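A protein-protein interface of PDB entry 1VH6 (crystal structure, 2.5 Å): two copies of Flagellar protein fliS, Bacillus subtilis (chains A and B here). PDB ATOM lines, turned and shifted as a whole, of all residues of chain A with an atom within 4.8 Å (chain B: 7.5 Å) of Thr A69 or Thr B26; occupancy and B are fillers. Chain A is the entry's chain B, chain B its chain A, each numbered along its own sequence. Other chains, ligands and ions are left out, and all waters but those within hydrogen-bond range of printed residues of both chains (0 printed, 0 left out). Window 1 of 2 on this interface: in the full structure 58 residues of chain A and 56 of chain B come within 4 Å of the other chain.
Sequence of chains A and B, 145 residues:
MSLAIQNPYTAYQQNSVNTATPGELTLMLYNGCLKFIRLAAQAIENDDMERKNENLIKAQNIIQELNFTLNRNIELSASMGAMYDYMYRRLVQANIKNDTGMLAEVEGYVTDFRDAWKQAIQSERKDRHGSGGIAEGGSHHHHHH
O of Gly B23 sits at hydrogen-bond distance from NE1 of Trp A117, at 2.9 Å. N of Gly B23 is in hydrogen-bond range of OE1 of Glu A65, 3.1 Å away. The side-chain hydroxyl of Thr B26 lies within hydrogen-bond range of the side-chain hydroxyl of Thr A69, at 3.5 Å. The side-chain amide nitrogen of Asn A73 lies within hydrogen-bond range of the side-chain amide oxygen of Asn B73, at 3.3 Å.
O of Asn A67 is in hydrogen-bond range of ND2 of Asn A71. O of Glu A65 lies within hydrogen-bond range of OG1 of Thr A69 (3.1 Å). O of Thr B69 lies close to ND2 of Asn B73, 3.1 Å away. O of Thr A69 lies close to ND2 of Asn A73 (3.3 Å).
Pro B22 touches Glu A65 (CA to OE1, 3.99 Å). Glu A65 touches Leu B25. Tyr B84 touches Asn A67. Phe A68 touches Gly B23 (CD2 to CA, 3.6 Å). CG2 of Thr A69 touches OD1 of Asn B73 (3.8 Å). CD1 of Leu A70 touches O of Asn B73, 3.3 Å away. CA of Leu B70 touches ND2 of Asn A73, 3.6 Å away. Thr B26 touches Trp A117. N of Leu B27 touches NE1 of Trp A117 (3.9 Å). Tyr B30 touches Trp A117.
Of chain B, only Thr B26 and Asn B73 come within 4 Å of Thr A69. Of chain A, only Thr A69 (3.5 Å) and Trp A117 (3.3 Å) come within 4 Å of Thr B26. Of the printed residues of chain A, Pro B22 touches Glu A65 and Phe A68. Of the printed residues of chain B, Trp A117 touches Gly B23 (2.9 Å), Thr B26 (3.3 Å), Leu B27 (3.9 Å) and Tyr B30 (3.99 Å).
Of the 10 printed residues of chain A, 8 touch a printed residue of chain B. Hydrophobic or aromatic side chains of chain A within 4 Å of the printed part of chain B: Leu A66, Phe A68, Leu A70 and Trp A117. Along chain A the printed residues that touch a printed residue of chain B span positions 65 to 117. Among the printed residues, 17 pairs touch across the chains. Among the printed residues, no Asp or Glu carboxylate lies within 4 Å of a Lys or Arg side-chain nitrogen of the other chain.
Thr A69 touches Asn B73, but with the chains exchanged Asn A73 does not touch Thr B69 (4.1 Å). Leu A70 touches Asn B73, and with the chains exchanged Asn A73 touches Leu B70. Asn A73 touches its own counterpart, Asn B73. Positions printed for both chains: 66, 69, 70 and 73. Of the 17 pairs that touch across the chains among the printed residues, 3 have their exchanged pair printed and touching as well.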
ATOM      1  N   GLU A  65     -10.828 -28.405  22.450  1.00  0.00           N
ATOM      2  CA  GLU A  65      -9.577 -27.878  21.906  1.00  0.00           C
ATOM      3  C   GLU A  65      -8.928 -26.985  22.959  1.00  0.00           C
ATOM      4  O   GLU A  65      -7.716 -27.031  23.178  1.00  0.00           O
ATOM      5  CB  GLU A  65      -9.853 -27.069  20.638  1.00  0.00           C
ATOM      6  CG  GLU A  65      -8.640 -26.386  20.030  1.00  0.00           C
ATOM      7  CD  GLU A  65      -7.558 -27.363  19.621  1.00  0.00           C
ATOM      8  OE1 GLU A  65      -7.856 -28.332  18.892  1.00  0.00           O
ATOM      9  OE2 GLU A  65      -6.397 -27.158  20.029  1.00  0.00           O
ATOM     10  N   LEU A  66      -9.749 -26.172  23.614  1.00  0.00           N
ATOM     11  CA  LEU A  66      -9.267 -25.272  24.652  1.00  0.00           C
ATOM     12  C   LEU A  66      -8.859 -26.078  25.868  1.00  0.00           C
ATOM     13  O   LEU A  66      -7.827 -25.806  26.495  1.00  0.00           O
ATOM     14  CB  LEU A  66     -10.365 -24.283  25.050  1.00  0.00           C
ATOM     15  CG  LEU A  66     -10.698 -23.274  23.957  1.00  0.00           C
ATOM     16  CD1 LEU A  66     -11.990 -22.518  24.297  1.00  0.00           C
ATOM     17  CD2 LEU A  66      -9.508 -22.327  23.796  1.00  0.00           C
ATOM     18  N   ASN A  67      -9.684 -27.068  26.198  1.00  0.00           N
ATOM     19  CA  ASN A  67      -9.440 -27.926  27.350  1.00  0.00           C
ATOM     20  C   ASN A  67      -8.106 -28.654  27.228  1.00  0.00           C
ATOM     21  O   ASN A  67      -7.330 -28.701  28.182  1.00  0.00           O
ATOM     22  CB  ASN A  67     -10.574 -28.941  27.490  1.00  0.00           C
ATOM     23  CG  ASN A  67     -10.584 -29.617  28.844  1.00  0.00           C
ATOM     24  OD1 ASN A  67     -10.674 -30.837  28.932  1.00  0.00           O
ATOM     25  ND2 ASN A  67     -10.474 -28.829  29.908  1.00  0.00           N
ATOM     26  N   PHE A  68      -7.836 -29.200  26.046  1.00  0.00           N
ATOM     27  CA  PHE A  68      -6.592 -29.920  25.820  1.00  0.00           C
ATOM     28  C   PHE A  68      -5.380 -29.019  25.975  1.00  0.00           C
ATOM     29  O   PHE A  68      -4.423 -29.363  26.671  1.00  0.00           O
ATOM     30  CB  PHE A  68      -6.553 -30.528  24.423  1.00  0.00           C
ATOM     31  CG  PHE A  68      -5.362 -31.397  24.196  1.00  0.00           C
ATOM     32  CD1 PHE A  68      -5.382 -32.732  24.576  1.00  0.00           C
ATOM     33  CD2 PHE A  68      -4.185 -30.859  23.687  1.00  0.00           C
ATOM     34  CE1 PHE A  68      -4.240 -33.516  24.461  1.00  0.00           C
ATOM     35  CE2 PHE A  68      -3.039 -31.637  23.571  1.00  0.00           C
ATOM     36  CZ  PHE A  68      -3.065 -32.967  23.961  1.00  0.00           C
ATOM     37  N   THR A  69      -5.425 -27.869  25.309  1.00  0.00           N
ATOM     38  CA  THR A  69      -4.333 -26.912  25.362  1.00  0.00           C
ATOM     39  C   THR A  69      -4.098 -26.372  26.764  1.00  0.00           C
ATOM     40  O   THR A  69      -2.958 -26.230  27.186  1.00  0.00           O
ATOM     41  CB  THR A  69      -4.583 -25.736  24.399  1.00  0.00           C
ATOM     42  OG1 THR A  69      -4.671 -26.241  23.065  1.00  0.00           O
ATOM     43  CG2 THR A  69      -3.434 -24.724  24.464  1.00  0.00           C
ATOM     44  N   LEU A  70      -5.169 -26.072  27.486  1.00  0.00           N
ATOM     45  CA  LEU A  70      -5.034 -25.552  28.845  1.00  0.00           C
ATOM     46  C   LEU A  70      -4.293 -26.551  29.717  1.00  0.00           C
ATOM     47  O   LEU A  70      -3.301 -26.218  30.370  1.00  0.00           O
ATOM     48  CB  LEU A  70      -6.409 -25.288  29.459  1.00  0.00           C
ATOM     49  CG  LEU A  70      -6.476 -24.999  30.961  1.00  0.00           C
ATOM     50  CD1 LEU A  70      -6.410 -23.505  31.215  1.00  0.00           C
ATOM     51  CD2 LEU A  70      -7.774 -25.555  31.512  1.00  0.00           C
ATOM     52  N   ASN A  71      -4.779 -27.786  29.721  1.00  0.00           N
ATOM     53  CA  ASN A  71      -4.171 -28.816  30.542  1.00  0.00           C
ATOM     54  C   ASN A  71      -2.723 -29.102  30.190  1.00  0.00           C
ATOM     55  O   ASN A  71      -1.888 -29.209  31.072  1.00  0.00           O
ATOM     56  CB  ASN A  71      -5.012 -30.095  30.492  1.00  0.00           C
ATOM     57  CG  ASN A  71      -6.355 -29.915  31.162  1.00  0.00           C
ATOM     58  OD1 ASN A  71      -6.430 -29.463  32.306  1.00  0.00           O
ATOM     59  ND2 ASN A  71      -7.427 -30.262  30.454  1.00  0.00           N
ATOM     60  N   ARG A  72      -2.413 -29.216  28.907  1.00  0.00           N
ATOM     61  CA  ARG A  72      -1.033 -29.485  28.535  1.00  0.00           C
ATOM     62  C   ARG A  72      -0.151 -28.296  28.880  1.00  0.00           C
ATOM     63  O   ARG A  72       0.979 -28.477  29.322  1.00  0.00           O
ATOM     64  CB  ARG A  72      -0.896 -29.806  27.047  1.00  0.00           C
ATOM     65  CG  ARG A  72       0.561 -30.035  26.657  1.00  0.00           C
ATOM     66  CD  ARG A  72       0.724 -30.690  25.301  1.00  0.00           C
ATOM     67  NE  ARG A  72       2.123 -31.026  25.053  1.00  0.00           N
ATOM     68  CZ  ARG A  72       2.838 -31.880  25.786  1.00  0.00           C
ATOM     69  NH1 ARG A  72       2.284 -32.497  26.825  1.00  0.00           N
ATOM     70  NH2 ARG A  72       4.111 -32.107  25.485  1.00  0.00           N
ATOM     71  N   ASN A  73      -0.665 -27.085  28.688  1.00  0.00           N
ATOM     72  CA  ASN A  73       0.112 -25.892  28.995  1.00  0.00           C
ATOM     73  C   ASN A  73       0.426 -25.772  30.477  1.00  0.00           C
ATOM     74  O   ASN A  73       1.489 -25.269  30.842  1.00  0.00           O
ATOM     75  CB  ASN A  73      -0.597 -24.627  28.502  1.00  0.00           C
ATOM     76  CG  ASN A  73      -0.303 -24.332  27.038  1.00  0.00           C
ATOM     77  OD1 ASN A  73       0.688 -24.820  26.491  1.00  0.00           O
ATOM     78  ND2 ASN A  73      -1.147 -23.528  26.405  1.00  0.00           N
ATOM     79  N   TRP A 117       4.276 -32.447  21.151  1.00  0.00           N
ATOM     80  CA  TRP A 117       2.860 -32.087  21.181  1.00  0.00           C
ATOM     81  C   TRP A 117       2.041 -33.094  20.376  1.00  0.00           C
ATOM     82  O   TRP A 117       0.924 -33.452  20.757  1.00  0.00           O
ATOM     83  CB  TRP A 117       2.663 -30.683  20.601  1.00  0.00           C
ATOM     84  CG  TRP A 117       1.273 -30.152  20.786  1.00  0.00           C
ATOM     85  CD1 TRP A 117       0.168 -30.463  20.048  1.00  0.00           C
ATOM     86  CD2 TRP A 117       0.828 -29.266  21.825  1.00  0.00           C
ATOM     87  NE1 TRP A 117      -0.939 -29.830  20.564  1.00  0.00           N
ATOM     88  CE2 TRP A 117      -0.563 -29.091  21.656  1.00  0.00           C
ATOM     89  CE3 TRP A 117       1.472 -28.607  22.882  1.00  0.00           C
ATOM     90  CZ2 TRP A 117      -1.326 -28.287  22.508  1.00  0.00           C
ATOM     91  CZ3 TRP A 117       0.707 -27.803  23.736  1.00  0.00           C
ATOM     92  CH2 TRP A 117      -0.674 -27.651  23.540  1.00  0.00           C
ATOM     93  N   PRO B  22      -8.628 -33.076  19.592  1.00  0.00           N
ATOM     94  CA  PRO B  22      -8.219 -31.976  20.473  1.00  0.00           C
ATOM     95  C   PRO B  22      -6.695 -31.781  20.547  1.00  0.00           C
ATOM     96  O   PRO B  22      -5.955 -32.678  20.947  1.00  0.00           O
ATOM     97  CB  PRO B  22      -8.866 -32.342  21.820  1.00  0.00           C
ATOM     98  CG  PRO B  22      -9.139 -33.834  21.709  1.00  0.00           C
ATOM     99  CD  PRO B  22      -9.535 -34.015  20.275  1.00  0.00           C
ATOM    100  N   GLY B  23      -6.234 -30.603  20.139  1.00  0.00           N
ATOM    101  CA  GLY B  23      -4.813 -30.314  20.164  1.00  0.00           C
ATOM    102  C   GLY B  23      -4.250 -29.953  18.804  1.00  0.00           C
ATOM    103  O   GLY B  23      -3.146 -29.421  18.710  1.00  0.00           O
ATOM    104  N   GLU B  24      -5.016 -30.235  17.752  1.00  0.00           N
ATOM    105  CA  GLU B  24      -4.612 -29.951  16.375  1.00  0.00           C
ATOM    106  C   GLU B  24      -4.125 -28.534  16.104  1.00  0.00           C
ATOM    107  O   GLU B  24      -3.095 -28.347  15.467  1.00  0.00           O
ATOM    108  CB  GLU B  24      -5.772 -30.177  15.414  1.00  0.00           C
ATOM    109  CG  GLU B  24      -6.508 -31.452  15.580  1.00  0.00           C
ATOM    110  CD  GLU B  24      -7.746 -31.480  14.728  1.00  0.00           C
ATOM    111  OE1 GLU B  24      -7.601 -31.654  13.503  1.00  0.00           O
ATOM    112  OE2 GLU B  24      -8.854 -31.315  15.275  1.00  0.00           O
ATOM    113  N   LEU B  25      -4.895 -27.542  16.548  1.00  0.00           N
ATOM    114  CA  LEU B  25      -4.565 -26.141  16.296  1.00  0.00           C
ATOM    115  C   LEU B  25      -3.190 -25.715  16.785  1.00  0.00           C
ATOM    116  O   LEU B  25      -2.519 -24.931  16.121  1.00  0.00           O
ATOM    117  CB  LEU B  25      -5.662 -25.210  16.856  1.00  0.00           C
ATOM    118  CG  LEU B  25      -7.051 -25.308  16.183  1.00  0.00           C
ATOM    119  CD1 LEU B  25      -7.963 -24.161  16.612  1.00  0.00           C
ATOM    120  CD2 LEU B  25      -6.890 -25.263  14.671  1.00  0.00           C
ATOM    121  N   THR B  26      -2.752 -26.230  17.928  1.00  0.00           N
ATOM    122  CA  THR B  26      -1.426 -25.868  18.422  1.00  0.00           C
ATOM    123  C   THR B  26      -0.384 -26.587  17.567  1.00  0.00           C
ATOM    124  O   THR B  26       0.672 -26.043  17.257  1.00  0.00           O
ATOM    125  CB  THR B  26      -1.247 -26.257  19.897  1.00  0.00           C
ATOM    126  OG1 THR B  26      -2.208 -25.548  20.689  1.00  0.00           O
ATOM    127  CG2 THR B  26       0.155 -25.903  20.376  1.00  0.00           C
ATOM    128  N   LEU B  27      -0.690 -27.823  17.189  1.00  0.00           N
ATOM    129  CA  LEU B  27       0.206 -28.583  16.339  1.00  0.00           C
ATOM    130  C   LEU B  27       0.353 -27.751  15.064  1.00  0.00           C
ATOM    131  O   LEU B  27       1.451 -27.550  14.546  1.00  0.00           O
ATOM    132  CB  LEU B  27      -0.404 -29.947  16.016  1.00  0.00           C
ATOM    133  CG  LEU B  27       0.409 -30.855  15.086  1.00  0.00           C
ATOM    134  CD1 LEU B  27       1.792 -31.099  15.677  1.00  0.00           C
ATOM    135  CD2 LEU B  27      -0.337 -32.166  14.877  1.00  0.00           C
ATOM    136  N   MET B  28      -0.769 -27.244  14.581  1.00  0.00           N
ATOM    137  CA  MET B  28      -0.774 -26.427  13.386  1.00  0.00           C
ATOM    138  C   MET B  28       0.108 -25.183  13.538  1.00  0.00           C
ATOM    139  O   MET B  28       0.832 -24.815  12.617  1.00  0.00           O
ATOM    140  CB  MET B  28      -2.200 -26.020  13.066  1.00  0.00           C
ATOM    141  CG  MET B  28      -2.346 -25.239  11.792  1.00  0.00           C
ATOM    142  SD  MET B  28      -4.195 -24.778  11.582  1.00  0.00           S
ATOM    143  CE  MET B  28      -4.902 -26.574  11.311  1.00  0.00           C
ATOM    144  N   LEU B  29       0.046 -24.526  14.691  1.00  0.00           N
ATOM    145  CA  LEU B  29       0.874 -23.343  14.905  1.00  0.00           C
ATOM    146  C   LEU B  29       2.361 -23.719  14.860  1.00  0.00           C
ATOM    147  O   LEU B  29       3.166 -23.023  14.239  1.00  0.00           O
ATOM    148  CB  LEU B  29       0.544 -22.683  16.248  1.00  0.00           C
ATOM    149  CG  LEU B  29      -0.866 -22.118  16.429  1.00  0.00           C
ATOM    150  CD1 LEU B  29      -0.924 -21.350  17.741  1.00  0.00           C
ATOM    151  CD2 LEU B  29      -1.226 -21.199  15.262  1.00  0.00           C
ATOM    152  N   TYR B  30       2.715 -24.822  15.517  1.00  0.00           N
ATOM    153  CA  TYR B  30       4.100 -25.294  15.530  1.00  0.00           C
ATOM    154  C   TYR B  30       4.602 -25.579  14.124  1.00  0.00           C
ATOM    155  O   TYR B  30       5.701 -25.176  13.762  1.00  0.00           O
ATOM    156  CB  TYR B  30       4.228 -26.560  16.373  1.00  0.00           C
ATOM    157  CG  TYR B  30       4.333 -26.288  17.847  1.00  0.00           C
ATOM    158  CD1 TYR B  30       3.444 -26.867  18.747  1.00  0.00           C
ATOM    159  CD2 TYR B  30       5.321 -25.451  18.345  1.00  0.00           C
ATOM    160  CE1 TYR B  30       3.541 -26.617  20.108  1.00  0.00           C
ATOM    161  CE2 TYR B  30       5.425 -25.196  19.698  1.00  0.00           C
ATOM    162  CZ  TYR B  30       4.535 -25.781  20.571  1.00  0.00           C
ATOM    163  OH  TYR B  30       4.642 -25.535  21.915  1.00  0.00           O
ATOM    164  N   ASN B  31       3.797 -26.283  13.335  1.00  0.00           N
ATOM    165  CA  ASN B  31       4.172 -26.598  11.963  1.00  0.00           C
ATOM    166  C   ASN B  31       4.266 -25.320  11.140  1.00  0.00           C
ATOM    167  O   ASN B  31       5.169 -25.175  10.324  1.00  0.00           O
ATOM    168  CB  ASN B  31       3.172 -27.577  11.336  1.00  0.00           C
ATOM    169  CG  ASN B  31       3.370 -29.004  11.836  1.00  0.00           C
ATOM    170  OD1 ASN B  31       4.496 -29.415  12.114  1.00  0.00           O
ATOM    171  ND2 ASN B  31       2.291 -29.765  11.935  1.00  0.00           N
ATOM    172  N   GLY B  32       3.339 -24.391  11.359  1.00  0.00           N
ATOM    173  CA  GLY B  32       3.397 -23.137  10.638  1.00  0.00           C
ATOM    174  C   GLY B  32       4.708 -22.440  10.970  1.00  0.00           C
ATOM    175  O   GLY B  32       5.427 -21.975  10.083  1.00  0.00           O
ATOM    176  N   ILE B  62       3.696 -16.276  15.749  1.00  0.00           N
ATOM    177  CA  ILE B  62       3.238 -17.579  16.200  1.00  0.00           C
ATOM    178  C   ILE B  62       3.759 -17.857  17.600  1.00  0.00           C
ATOM    179  O   ILE B  62       3.018 -18.336  18.450  1.00  0.00           O
ATOM    180  CB  ILE B  62       3.669 -18.701  15.225  1.00  0.00           C
ATOM    181  CG1 ILE B  62       2.837 -18.593  13.944  1.00  0.00           C
ATOM    182  CG2 ILE B  62       3.450 -20.066  15.865  1.00  0.00           C
ATOM    183  CD1 ILE B  62       3.320 -19.453  12.794  1.00  0.00           C
ATOM    184  N   LEU B  66       1.548 -18.527  20.988  1.00  0.00           N
ATOM    185  CA  LEU B  66       1.674 -19.688  21.858  1.00  0.00           C
ATOM    186  C   LEU B  66       2.062 -19.269  23.269  1.00  0.00           C
ATOM    187  O   LEU B  66       1.622 -19.870  24.250  1.00  0.00           O
ATOM    188  CB  LEU B  66       2.749 -20.641  21.327  1.00  0.00           C
ATOM    189  CG  LEU B  66       2.488 -21.380  20.019  1.00  0.00           C
ATOM    190  CD1 LEU B  66       3.798 -21.937  19.467  1.00  0.00           C
ATOM    191  CD2 LEU B  66       1.453 -22.489  20.260  1.00  0.00           C
ATOM    192  N   THR B  69      -1.073 -17.559  25.116  1.00  0.00           N
ATOM    193  CA  THR B  69      -2.015 -18.589  25.524  1.00  0.00           C
ATOM    194  C   THR B  69      -1.508 -19.375  26.726  1.00  0.00           C
ATOM    195  O   THR B  69      -2.237 -19.579  27.697  1.00  0.00           O
ATOM    196  CB  THR B  69      -2.305 -19.560  24.372  1.00  0.00           C
ATOM    197  OG1 THR B  69      -2.746 -18.813  23.231  1.00  0.00           O
ATOM    198  CG2 THR B  69      -3.396 -20.557  24.770  1.00  0.00           C
ATOM    199  N   LEU B  70      -0.258 -19.816  26.659  1.00  0.00           N
ATOM    200  CA  LEU B  70       0.329 -20.565  27.759  1.00  0.00           C
ATOM    201  C   LEU B  70       0.290 -19.778  29.076  1.00  0.00           C
ATOM    202  O   LEU B  70      -0.134 -20.310  30.101  1.00  0.00           O
ATOM    203  CB  LEU B  70       1.777 -20.947  27.423  1.00  0.00           C
ATOM    204  CG  LEU B  70       2.564 -21.696  28.506  1.00  0.00           C
ATOM    205  CD1 LEU B  70       3.604 -22.577  27.841  1.00  0.00           C
ATOM    206  CD2 LEU B  70       3.219 -20.718  29.463  1.00  0.00           C
ATOM    207  N   ASN B  73      -3.372 -19.552  30.333  1.00  0.00           N
ATOM    208  CA  ASN B  73      -3.852 -20.861  30.780  1.00  0.00           C
ATOM    209  C   ASN B  73      -3.310 -21.280  32.134  1.00  0.00           C
ATOM    210  O   ASN B  73      -3.940 -22.053  32.840  1.00  0.00           O
ATOM    211  CB  ASN B  73      -3.511 -21.944  29.758  1.00  0.00           C
ATOM    212  CG  ASN B  73      -4.262 -21.772  28.455  1.00  0.00           C
ATOM    213  OD1 ASN B  73      -4.136 -22.593  27.547  1.00  0.00           O
ATOM    214  ND2 ASN B  73      -5.043 -20.705  28.353  1.00  0.00           N
ATOM    215  N   TYR B  84     -14.463 -26.520  31.764  1.00  0.00           N
ATOM    216  CA  TYR B  84     -14.546 -26.929  30.370  1.00  0.00           C
ATOM    217  C   TYR B  84     -15.235 -28.286  30.265  1.00  0.00           C
ATOM    218  O   TYR B  84     -15.994 -28.525  29.332  1.00  0.00           O
ATOM    219  CB  TYR B  84     -13.150 -26.993  29.742  1.00  0.00           C
ATOM    220  CG  TYR B  84     -12.629 -25.654  29.272  1.00  0.00           C
ATOM    221  CD1 TYR B  84     -11.267 -25.353  29.329  1.00  0.00           C
ATOM    222  CD2 TYR B  84     -13.495 -24.693  28.744  1.00  0.00           C
ATOM    223  CE1 TYR B  84     -10.776 -24.128  28.872  1.00  0.00           C
ATOM    224  CE2 TYR B  84     -13.018 -23.464  28.283  1.00  0.00           C
ATOM    225  CZ  TYR B  84     -11.656 -23.190  28.349  1.00  0.00           C
ATOM    226  OH  TYR B  84     -11.171 -21.991  27.875  1.00  0.00           O
